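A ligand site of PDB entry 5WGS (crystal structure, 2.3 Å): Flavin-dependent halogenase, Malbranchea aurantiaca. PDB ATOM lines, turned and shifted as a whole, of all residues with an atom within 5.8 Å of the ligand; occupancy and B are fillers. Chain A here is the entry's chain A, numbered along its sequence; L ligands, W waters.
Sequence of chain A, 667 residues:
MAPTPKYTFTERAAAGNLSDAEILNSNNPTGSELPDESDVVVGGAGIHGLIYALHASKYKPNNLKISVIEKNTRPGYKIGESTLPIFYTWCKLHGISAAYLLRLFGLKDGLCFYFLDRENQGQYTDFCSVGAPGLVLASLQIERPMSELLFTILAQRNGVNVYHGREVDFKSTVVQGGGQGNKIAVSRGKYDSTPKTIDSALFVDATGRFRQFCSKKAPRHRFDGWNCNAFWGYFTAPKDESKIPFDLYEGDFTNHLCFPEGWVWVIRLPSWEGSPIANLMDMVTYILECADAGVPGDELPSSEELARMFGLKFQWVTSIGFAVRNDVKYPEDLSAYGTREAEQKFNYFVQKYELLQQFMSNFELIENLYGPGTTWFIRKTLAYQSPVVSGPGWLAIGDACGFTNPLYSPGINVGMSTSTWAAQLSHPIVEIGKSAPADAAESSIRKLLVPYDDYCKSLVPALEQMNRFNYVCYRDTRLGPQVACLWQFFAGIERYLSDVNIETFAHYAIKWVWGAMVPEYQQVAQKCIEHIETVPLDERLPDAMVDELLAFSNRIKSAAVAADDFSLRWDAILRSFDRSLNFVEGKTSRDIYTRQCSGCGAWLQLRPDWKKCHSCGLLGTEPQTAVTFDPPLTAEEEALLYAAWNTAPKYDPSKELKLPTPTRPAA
N2 of the ligand sits at hydrogen-bond distance from OE1 of Glu 494, 2.5 Å away. N1 of the ligand lies close to O of Gly 131 (3.1 Å).
N of Val 130 is in hydrogen-bond range of O of Ile 573 (3.2 Å). The backbone carbonyl oxygen (O) of Ile 493 is in hydrogen-bond range of the guanidinium group (NH1) of Arg 495 (3.4 Å). The backbone carbonyl oxygen (O) of Ser 129 lies within hydrogen-bond range of the backbone NH (N) of Leu 111 (3.0 Å).
Merely in contact with the ligand: Val 130, Pro 133, Trp 645, Phe 489, Ala 132, Pro 85, Leu 137, Val 136, Leu 641, Ile 493, Ile 573, Ser 129 and Leu 568. Hydrophobic or aromatic side chains that line the ligand: Pro 85, Ala 132, Pro 133, Val 136, Leu 137, Phe 489, Ile 493, Leu 568, Ile 573, Leu 641 and Trp 645. 15 residues have an atom within 4 Å of the ligand: Pro 85, Ser 129, Val 130, Gly 131, Ala 132, Pro 133, Val 136, Leu 137, Phe 489, Ile 493, Glu 494, Leu 568, Ile 573, Leu 641 and Trp 645. Along chain A the residues within 4 Å of the ligand span positions 85 to 645.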
ATOM      1  N   PRO A  85     -16.106  20.122 -13.625  1.00  0.00           N
ATOM      2  CA  PRO A  85     -15.006  19.138 -13.443  1.00  0.00           C
ATOM      3  C   PRO A  85     -14.048  18.995 -14.613  1.00  0.00           C
ATOM      4  O   PRO A  85     -12.845  18.810 -14.389  1.00  0.00           O
ATOM      5  CB  PRO A  85     -15.777  17.832 -13.181  1.00  0.00           C
ATOM      6  CG  PRO A  85     -17.052  18.267 -12.504  1.00  0.00           C
ATOM      7  CD  PRO A  85     -17.391  19.630 -13.084  1.00  0.00           C
ATOM      8  N   LEU A 111     -24.236  21.667  -8.436  1.00  0.00           N
ATOM      9  CA  LEU A 111     -25.284  22.528  -8.944  1.00  0.00           C
ATOM     10  C   LEU A 111     -26.561  22.274  -8.166  1.00  0.00           C
ATOM     11  O   LEU A 111     -26.914  21.128  -7.882  1.00  0.00           O
ATOM     12  CB  LEU A 111     -25.536  22.292 -10.439  1.00  0.00           C
ATOM     13  CG  LEU A 111     -24.456  22.739 -11.434  1.00  0.00           C
ATOM     14  CD1 LEU A 111     -23.326  21.701 -11.537  1.00  0.00           C
ATOM     15  CD2 LEU A 111     -25.059  23.034 -12.806  1.00  0.00           C
ATOM     16  N   SER A 129     -27.411  18.226  -7.123  1.00  0.00           N
ATOM     17  CA  SER A 129     -26.368  17.294  -7.530  1.00  0.00           C
ATOM     18  C   SER A 129     -25.043  17.797  -6.982  1.00  0.00           C
ATOM     19  O   SER A 129     -24.702  18.970  -7.166  1.00  0.00           O
ATOM     20  CB  SER A 129     -26.291  17.140  -9.051  1.00  0.00           C
ATOM     21  OG  SER A 129     -25.999  18.379  -9.661  1.00  0.00           O
ATOM     22  N   VAL A 130     -24.300  16.912  -6.315  1.00  0.00           N
ATOM     23  CA  VAL A 130     -23.106  17.264  -5.562  1.00  0.00           C
ATOM     24  C   VAL A 130     -21.853  17.193  -6.437  1.00  0.00           C
ATOM     25  O   VAL A 130     -21.912  16.807  -7.609  1.00  0.00           O
ATOM     26  CB  VAL A 130     -22.937  16.346  -4.345  1.00  0.00           C
ATOM     27  CG1 VAL A 130     -24.240  16.259  -3.572  1.00  0.00           C
ATOM     28  CG2 VAL A 130     -22.490  14.958  -4.795  1.00  0.00           C
ATOM     29  N   GLY A 131     -20.717  17.571  -5.861  1.00  0.00           N
ATOM     30  CA  GLY A 131     -19.428  17.457  -6.511  1.00  0.00           C
ATOM     31  C   GLY A 131     -18.709  16.151  -6.224  1.00  0.00           C
ATOM     32  O   GLY A 131     -19.224  15.084  -6.561  1.00  0.00           O
ATOM     33  N   ALA A 132     -17.538  16.215  -5.599  1.00  0.00           N
ATOM     34  CA  ALA A 132     -16.708  15.044  -5.379  1.00  0.00           C
ATOM     35  C   ALA A 132     -15.980  15.219  -4.050  1.00  0.00           C
ATOM     36  O   ALA A 132     -15.883  16.336  -3.529  1.00  0.00           O
ATOM     37  CB  ALA A 132     -15.701  14.858  -6.521  1.00  0.00           C
ATOM     38  N   PRO A 133     -15.470  14.120  -3.469  1.00  0.00           N
ATOM     39  CA  PRO A 133     -14.674  14.249  -2.234  1.00  0.00           C
ATOM     40  C   PRO A 133     -13.434  15.103  -2.437  1.00  0.00           C
ATOM     41  O   PRO A 133     -12.996  15.357  -3.564  1.00  0.00           O
ATOM     42  CB  PRO A 133     -14.291  12.791  -1.908  1.00  0.00           C
ATOM     43  CG  PRO A 133     -15.342  11.967  -2.545  1.00  0.00           C
ATOM     44  CD  PRO A 133     -15.767  12.716  -3.779  1.00  0.00           C
ATOM     45  N   VAL A 136     -10.808  13.535  -4.563  1.00  0.00           N
ATOM     46  CA  VAL A 136     -11.175  13.135  -5.919  1.00  0.00           C
ATOM     47  C   VAL A 136     -10.910  14.316  -6.857  1.00  0.00           C
ATOM     48  O   VAL A 136      -9.931  14.312  -7.608  1.00  0.00           O
ATOM     49  CB  VAL A 136     -12.644  12.668  -5.988  1.00  0.00           C
ATOM     50  CG1 VAL A 136     -13.095  12.480  -7.422  1.00  0.00           C
ATOM     51  CG2 VAL A 136     -12.797  11.358  -5.213  1.00  0.00           C
ATOM     52  N   LEU A 137     -11.752  15.346  -6.790  1.00  0.00           N
ATOM     53  CA  LEU A 137     -11.529  16.583  -7.526  1.00  0.00           C
ATOM     54  C   LEU A 137     -12.336  17.707  -6.875  1.00  0.00           C
ATOM     55  O   LEU A 137     -12.971  17.523  -5.836  1.00  0.00           O
ATOM     56  CB  LEU A 137     -11.870  16.430  -9.018  1.00  0.00           C
ATOM     57  CG  LEU A 137     -13.199  15.880  -9.545  1.00  0.00           C
ATOM     58  CD1 LEU A 137     -14.375  16.793  -9.246  1.00  0.00           C
ATOM     59  CD2 LEU A 137     -13.090  15.640 -11.047  1.00  0.00           C
ATOM     60  N   PHE A 489     -28.064  15.660 -16.350  1.00  0.00           N
ATOM     61  CA  PHE A 489     -27.013  14.990 -15.584  1.00  0.00           C
ATOM     62  C   PHE A 489     -26.835  13.542 -16.009  1.00  0.00           C
ATOM     63  O   PHE A 489     -25.709  13.031 -15.955  1.00  0.00           O
ATOM     64  CB  PHE A 489     -27.309  15.097 -14.095  1.00  0.00           C
ATOM     65  CG  PHE A 489     -27.141  16.489 -13.566  1.00  0.00           C
ATOM     66  CD1 PHE A 489     -25.897  16.936 -13.142  1.00  0.00           C
ATOM     67  CD2 PHE A 489     -28.208  17.371 -13.530  1.00  0.00           C
ATOM     68  CE1 PHE A 489     -25.736  18.231 -12.679  1.00  0.00           C
ATOM     69  CE2 PHE A 489     -28.053  18.660 -13.062  1.00  0.00           C
ATOM     70  CZ  PHE A 489     -26.817  19.093 -12.643  1.00  0.00           C
ATOM     71  N   GLY A 492     -25.116  13.988 -19.339  1.00  0.00           N
ATOM     72  CA  GLY A 492     -23.974  14.881 -19.343  1.00  0.00           C
ATOM     73  C   GLY A 492     -22.941  14.704 -18.259  1.00  0.00           C
ATOM     74  O   GLY A 492     -21.920  15.404 -18.247  1.00  0.00           O
ATOM     75  N   ILE A 493     -23.178  13.788 -17.314  1.00  0.00           N
ATOM     76  CA  ILE A 493     -22.150  13.501 -16.324  1.00  0.00           C
ATOM     77  C   ILE A 493     -20.930  12.914 -17.032  1.00  0.00           C
ATOM     78  O   ILE A 493     -21.048  12.152 -18.002  1.00  0.00           O
ATOM     79  CB  ILE A 493     -22.691  12.574 -15.222  1.00  0.00           C
ATOM     80  CG1 ILE A 493     -21.748  12.544 -14.021  1.00  0.00           C
ATOM     81  CG2 ILE A 493     -22.966  11.157 -15.748  1.00  0.00           C
ATOM     82  CD1 ILE A 493     -22.158  11.573 -12.962  1.00  0.00           C
ATOM     83  N   GLU A 494     -19.736  13.303 -16.560  1.00  0.00           N
ATOM     84  CA  GLU A 494     -18.488  13.100 -17.287  1.00  0.00           C
ATOM     85  C   GLU A 494     -17.893  11.734 -16.927  1.00  0.00           C
ATOM     86  O   GLU A 494     -16.981  11.608 -16.114  1.00  0.00           O
ATOM     87  CB  GLU A 494     -17.503  14.224 -16.990  1.00  0.00           C
ATOM     88  CG  GLU A 494     -18.079  15.644 -17.119  1.00  0.00           C
ATOM     89  CD  GLU A 494     -18.620  16.187 -15.801  1.00  0.00           C
ATOM     90  OE1 GLU A 494     -19.084  15.392 -14.962  1.00  0.00           O
ATOM     91  OE2 GLU A 494     -18.591  17.427 -15.603  1.00  0.00           O
ATOM     92  N   ARG A 495     -18.440  10.690 -17.556  1.00  0.00           N
ATOM     93  CA  ARG A 495     -17.961   9.347 -17.297  1.00  0.00           C
ATOM     94  C   ARG A 495     -16.504   9.187 -17.744  1.00  0.00           C
ATOM     95  O   ARG A 495     -16.097   9.705 -18.788  1.00  0.00           O
ATOM     96  CB  ARG A 495     -18.851   8.317 -18.015  1.00  0.00           C
ATOM     97  CG  ARG A 495     -20.349   8.346 -17.600  1.00  0.00           C
ATOM     98  CD  ARG A 495     -21.213   7.476 -18.539  1.00  0.00           C
ATOM     99  NE  ARG A 495     -22.629   7.446 -18.164  1.00  0.00           N
ATOM    100  CZ  ARG A 495     -23.483   8.445 -18.348  1.00  0.00           C
ATOM    101  NH1 ARG A 495     -23.064   9.586 -18.900  1.00  0.00           N
ATOM    102  NH2 ARG A 495     -24.758   8.326 -17.980  1.00  0.00           N
ATOM    103  N   LEU A 497     -13.748  10.498 -16.661  1.00  0.00           N
ATOM    104  CA  LEU A 497     -12.918  11.715 -16.701  1.00  0.00           C
ATOM    105  C   LEU A 497     -11.571  11.504 -16.017  1.00  0.00           C
ATOM    106  O   LEU A 497     -10.613  12.232 -16.324  1.00  0.00           O
ATOM    107  CB  LEU A 497     -13.661  12.889 -16.056  1.00  0.00           C
ATOM    108  CG  LEU A 497     -13.003  14.274 -15.870  1.00  0.00           C
ATOM    109  CD1 LEU A 497     -12.720  14.996 -17.182  1.00  0.00           C
ATOM    110  CD2 LEU A 497     -13.841  15.168 -14.948  1.00  0.00           C
ATOM    111  N   TRP A 514     -21.916  18.300 -22.813  1.00  0.00           N
ATOM    112  CA  TRP A 514     -22.898  18.257 -21.726  1.00  0.00           C
ATOM    113  C   TRP A 514     -23.992  17.207 -21.962  1.00  0.00           C
ATOM    114  O   TRP A 514     -25.080  17.292 -21.390  1.00  0.00           O
ATOM    115  CB  TRP A 514     -23.538  19.634 -21.492  1.00  0.00           C
ATOM    116  CG  TRP A 514     -23.223  20.240 -20.150  1.00  0.00           C
ATOM    117  CD1 TRP A 514     -22.520  21.391 -19.916  1.00  0.00           C
ATOM    118  CD2 TRP A 514     -23.588  19.725 -18.865  1.00  0.00           C
ATOM    119  NE1 TRP A 514     -22.426  21.618 -18.562  1.00  0.00           N
ATOM    120  CE2 TRP A 514     -23.070  20.610 -17.893  1.00  0.00           C
ATOM    121  CE3 TRP A 514     -24.295  18.593 -18.435  1.00  0.00           C
ATOM    122  CZ2 TRP A 514     -23.237  20.408 -16.515  1.00  0.00           C
ATOM    123  CZ3 TRP A 514     -24.469  18.390 -17.065  1.00  0.00           C
ATOM    124  CH2 TRP A 514     -23.933  19.297 -16.124  1.00  0.00           C
ATOM    125  N   PHE A 566     -21.998   2.140 -16.872  1.00  0.00           N
ATOM    126  CA  PHE A 566     -21.117   2.897 -15.990  1.00  0.00           C
ATOM    127  C   PHE A 566     -21.694   2.904 -14.581  1.00  0.00           C
ATOM    128  O   PHE A 566     -22.802   3.426 -14.359  1.00  0.00           O
ATOM    129  CB  PHE A 566     -20.923   4.317 -16.492  1.00  0.00           C
ATOM    130  CG  PHE A 566     -19.887   5.085 -15.731  1.00  0.00           C
ATOM    131  CD1 PHE A 566     -18.536   4.881 -15.965  1.00  0.00           C
ATOM    132  CD2 PHE A 566     -20.257   6.021 -14.780  1.00  0.00           C
ATOM    133  CE1 PHE A 566     -17.569   5.597 -15.259  1.00  0.00           C
ATOM    134  CE2 PHE A 566     -19.301   6.744 -14.079  1.00  0.00           C
ATOM    135  CZ  PHE A 566     -17.962   6.533 -14.314  1.00  0.00           C
ATOM    136  N   LEU A 568     -22.454   3.981 -10.964  1.00  0.00           N
ATOM    137  CA  LEU A 568     -22.498   5.210 -10.187  1.00  0.00           C
ATOM    138  C   LEU A 568     -23.407   5.015  -8.977  1.00  0.00           C
ATOM    139  O   LEU A 568     -24.407   4.288  -9.045  1.00  0.00           O
ATOM    140  CB  LEU A 568     -22.995   6.392 -11.024  1.00  0.00           C
ATOM    141  CG  LEU A 568     -21.904   7.091 -11.814  1.00  0.00           C
ATOM    142  CD1 LEU A 568     -22.482   7.875 -12.984  1.00  0.00           C
ATOM    143  CD2 LEU A 568     -21.121   8.018 -10.889  1.00  0.00           C
ATOM    144  N   ILE A 573     -25.505  11.072  -5.407  1.00  0.00           N
ATOM    145  CA  ILE A 573     -25.110  12.200  -6.241  1.00  0.00           C
ATOM    146  C   ILE A 573     -26.285  13.123  -6.526  1.00  0.00           C
ATOM    147  O   ILE A 573     -26.143  14.343  -6.489  1.00  0.00           O
ATOM    148  CB  ILE A 573     -24.479  11.664  -7.544  1.00  0.00           C
ATOM    149  CG1 ILE A 573     -23.164  10.964  -7.228  1.00  0.00           C
ATOM    150  CG2 ILE A 573     -24.282  12.776  -8.552  1.00  0.00           C
ATOM    151  CD1 ILE A 573     -22.584  10.213  -8.390  1.00  0.00           C
ATOM    152  N   LEU A 574     -27.463  12.550  -6.810  1.00  0.00           N
ATOM    153  CA  LEU A 574     -28.696  13.293  -6.963  1.00  0.00           C
ATOM    154  C   LEU A 574     -29.507  13.136  -5.682  1.00  0.00           C
ATOM    155  O   LEU A 574     -29.903  12.023  -5.325  1.00  0.00           O
ATOM    156  CB  LEU A 574     -29.498  12.810  -8.162  1.00  0.00           C
ATOM    157  CG  LEU A 574     -28.704  12.748  -9.462  1.00  0.00           C
ATOM    158  CD1 LEU A 574     -29.641  12.362 -10.605  1.00  0.00           C
ATOM    159  CD2 LEU A 574     -27.985  14.066  -9.733  1.00  0.00           C
ATOM    160  N   TYR A 593     -19.482  16.538   1.127  1.00  0.00           N
ATOM    161  CA  TYR A 593     -18.069  16.697   0.822  1.00  0.00           C
ATOM    162  C   TYR A 593     -17.498  18.020   1.327  1.00  0.00           C
ATOM    163  O   TYR A 593     -16.304  18.267   1.136  1.00  0.00           O
ATOM    164  CB  TYR A 593     -17.838  16.601  -0.691  1.00  0.00           C
ATOM    165  CG  TYR A 593     -18.277  15.291  -1.323  1.00  0.00           C
ATOM    166  CD1 TYR A 593     -18.017  14.075  -0.702  1.00  0.00           C
ATOM    167  CD2 TYR A 593     -18.952  15.282  -2.540  1.00  0.00           C
ATOM    168  CE1 TYR A 593     -18.419  12.881  -1.270  1.00  0.00           C
ATOM    169  CE2 TYR A 593     -19.355  14.094  -3.122  1.00  0.00           C
ATOM    170  CZ  TYR A 593     -19.080  12.892  -2.488  1.00  0.00           C
ATOM    171  OH  TYR A 593     -19.481  11.712  -3.058  1.00  0.00           O
ATOM    172  N   LEU A 641     -11.494   4.328  -4.457  1.00  0.00           N
ATOM    173  CA  LEU A 641     -11.972   5.500  -5.178  1.00  0.00           C
ATOM    174  C   LEU A 641     -10.900   6.575  -5.256  1.00  0.00           C
ATOM    175  O   LEU A 641     -10.575   7.066  -6.345  1.00  0.00           O
ATOM    176  CB  LEU A 641     -13.240   6.049  -4.504  1.00  0.00           C
ATOM    177  CG  LEU A 641     -13.862   7.264  -5.198  1.00  0.00           C
ATOM    178  CD1 LEU A 641     -14.564   6.842  -6.475  1.00  0.00           C
ATOM    179  CD2 LEU A 641     -14.811   8.012  -4.273  1.00  0.00           C
ATOM    180  N   TRP A 645      -8.185   8.776  -8.751  1.00  0.00           N
ATOM    181  CA  TRP A 645      -8.168  10.209  -9.009  1.00  0.00           C
ATOM    182  C   TRP A 645      -6.876  10.892  -8.567  1.00  0.00           C
ATOM    183  O   TRP A 645      -6.802  12.127  -8.606  1.00  0.00           O
ATOM    184  CB  TRP A 645      -9.363  10.868  -8.327  1.00  0.00           C
ATOM    185  CG  TRP A 645     -10.663  10.543  -8.991  1.00  0.00           C
ATOM    186  CD1 TRP A 645     -11.545   9.561  -8.637  1.00  0.00           C
ATOM    187  CD2 TRP A 645     -11.200  11.188 -10.146  1.00  0.00           C
ATOM    188  NE1 TRP A 645     -12.615   9.573  -9.501  1.00  0.00           N
ATOM    189  CE2 TRP A 645     -12.427  10.554 -10.436  1.00  0.00           C
ATOM    190  CE3 TRP A 645     -10.772  12.243 -10.963  1.00  0.00           C
ATOM    191  CZ2 TRP A 645     -13.234  10.947 -11.508  1.00  0.00           C
ATOM    192  CZ3 TRP A 645     -11.573  12.623 -12.025  1.00  0.00           C
ATOM    193  CH2 TRP A 645     -12.787  11.986 -12.287  1.00  0.00           C
HETATM  194  N1  LIG L   1     -18.120  12.450  -7.747  1.00  0.00           N
HETATM  195  C1  LIG L   1     -17.116  11.585  -7.571  1.00  0.00           C
HETATM  196  O1  LIG L   1     -16.546  11.398  -6.498  1.00  0.00           O
HETATM  197  C2  LIG L   1     -16.742  10.855  -8.862  1.00  0.00           C
HETATM  198  C3  LIG L   1     -22.565  16.937 -12.401  1.00  0.00           C
HETATM  199  C4  LIG L   1     -21.365  16.519 -12.949  1.00  0.00           C
HETATM  200  C5  LIG L   1     -20.560  15.662 -12.206  1.00  0.00           C
HETATM  201  C6  LIG L   1     -18.937  14.329 -11.438  1.00  0.00           C
HETATM  202  C7  LIG L   1     -17.628  13.564 -11.402  1.00  0.00           C
HETATM  203  C8  LIG L   1     -17.691  12.460 -12.469  1.00  0.00           C
HETATM  204  C9  LIG L   1     -16.500  14.535 -11.783  1.00  0.00           C
HETATM  205  C10 LIG L   1     -19.097  11.186  -9.573  1.00  0.00           C
HETATM  206  C11 LIG L   1     -17.455   9.374 -10.407  1.00  0.00           C
HETATM  207  C12 LIG L   1     -16.286   8.669  -9.726  1.00  0.00           C
HETATM  208  C13 LIG L   1     -16.308  11.940  -9.872  1.00  0.00           C
HETATM  209  C14 LIG L   1     -15.784   9.662  -8.684  1.00  0.00           C
HETATM  210  C15 LIG L   1     -17.413  13.015  -9.952  1.00  0.00           C
HETATM  211  C16 LIG L   1     -18.655  12.573  -9.108  1.00  0.00           C
HETATM  212  C17 LIG L   1     -19.743  13.662  -9.139  1.00  0.00           C
HETATM  213  C18 LIG L   1     -19.881  14.372 -10.457  1.00  0.00           C
HETATM  214  C19 LIG L   1     -20.941  15.212 -10.926  1.00  0.00           C
HETATM  215  C20 LIG L   1     -22.159  15.642 -10.404  1.00  0.00           C
HETATM  216  C21 LIG L   1     -22.962  16.508 -11.136  1.00  0.00           C
HETATM  217  N2  LIG L   1     -19.328  15.104 -12.505  1.00  0.00           N
HETATM  218  N3  LIG L   1     -17.993  10.247  -9.345  1.00  0.00           N
HETATM  219  O   HOH W   1     -14.392   6.530 -10.696  1.00  0.00           O
HETATM  220  O   HOH W   2     -18.481  16.743  -9.368  1.00  0.00           O
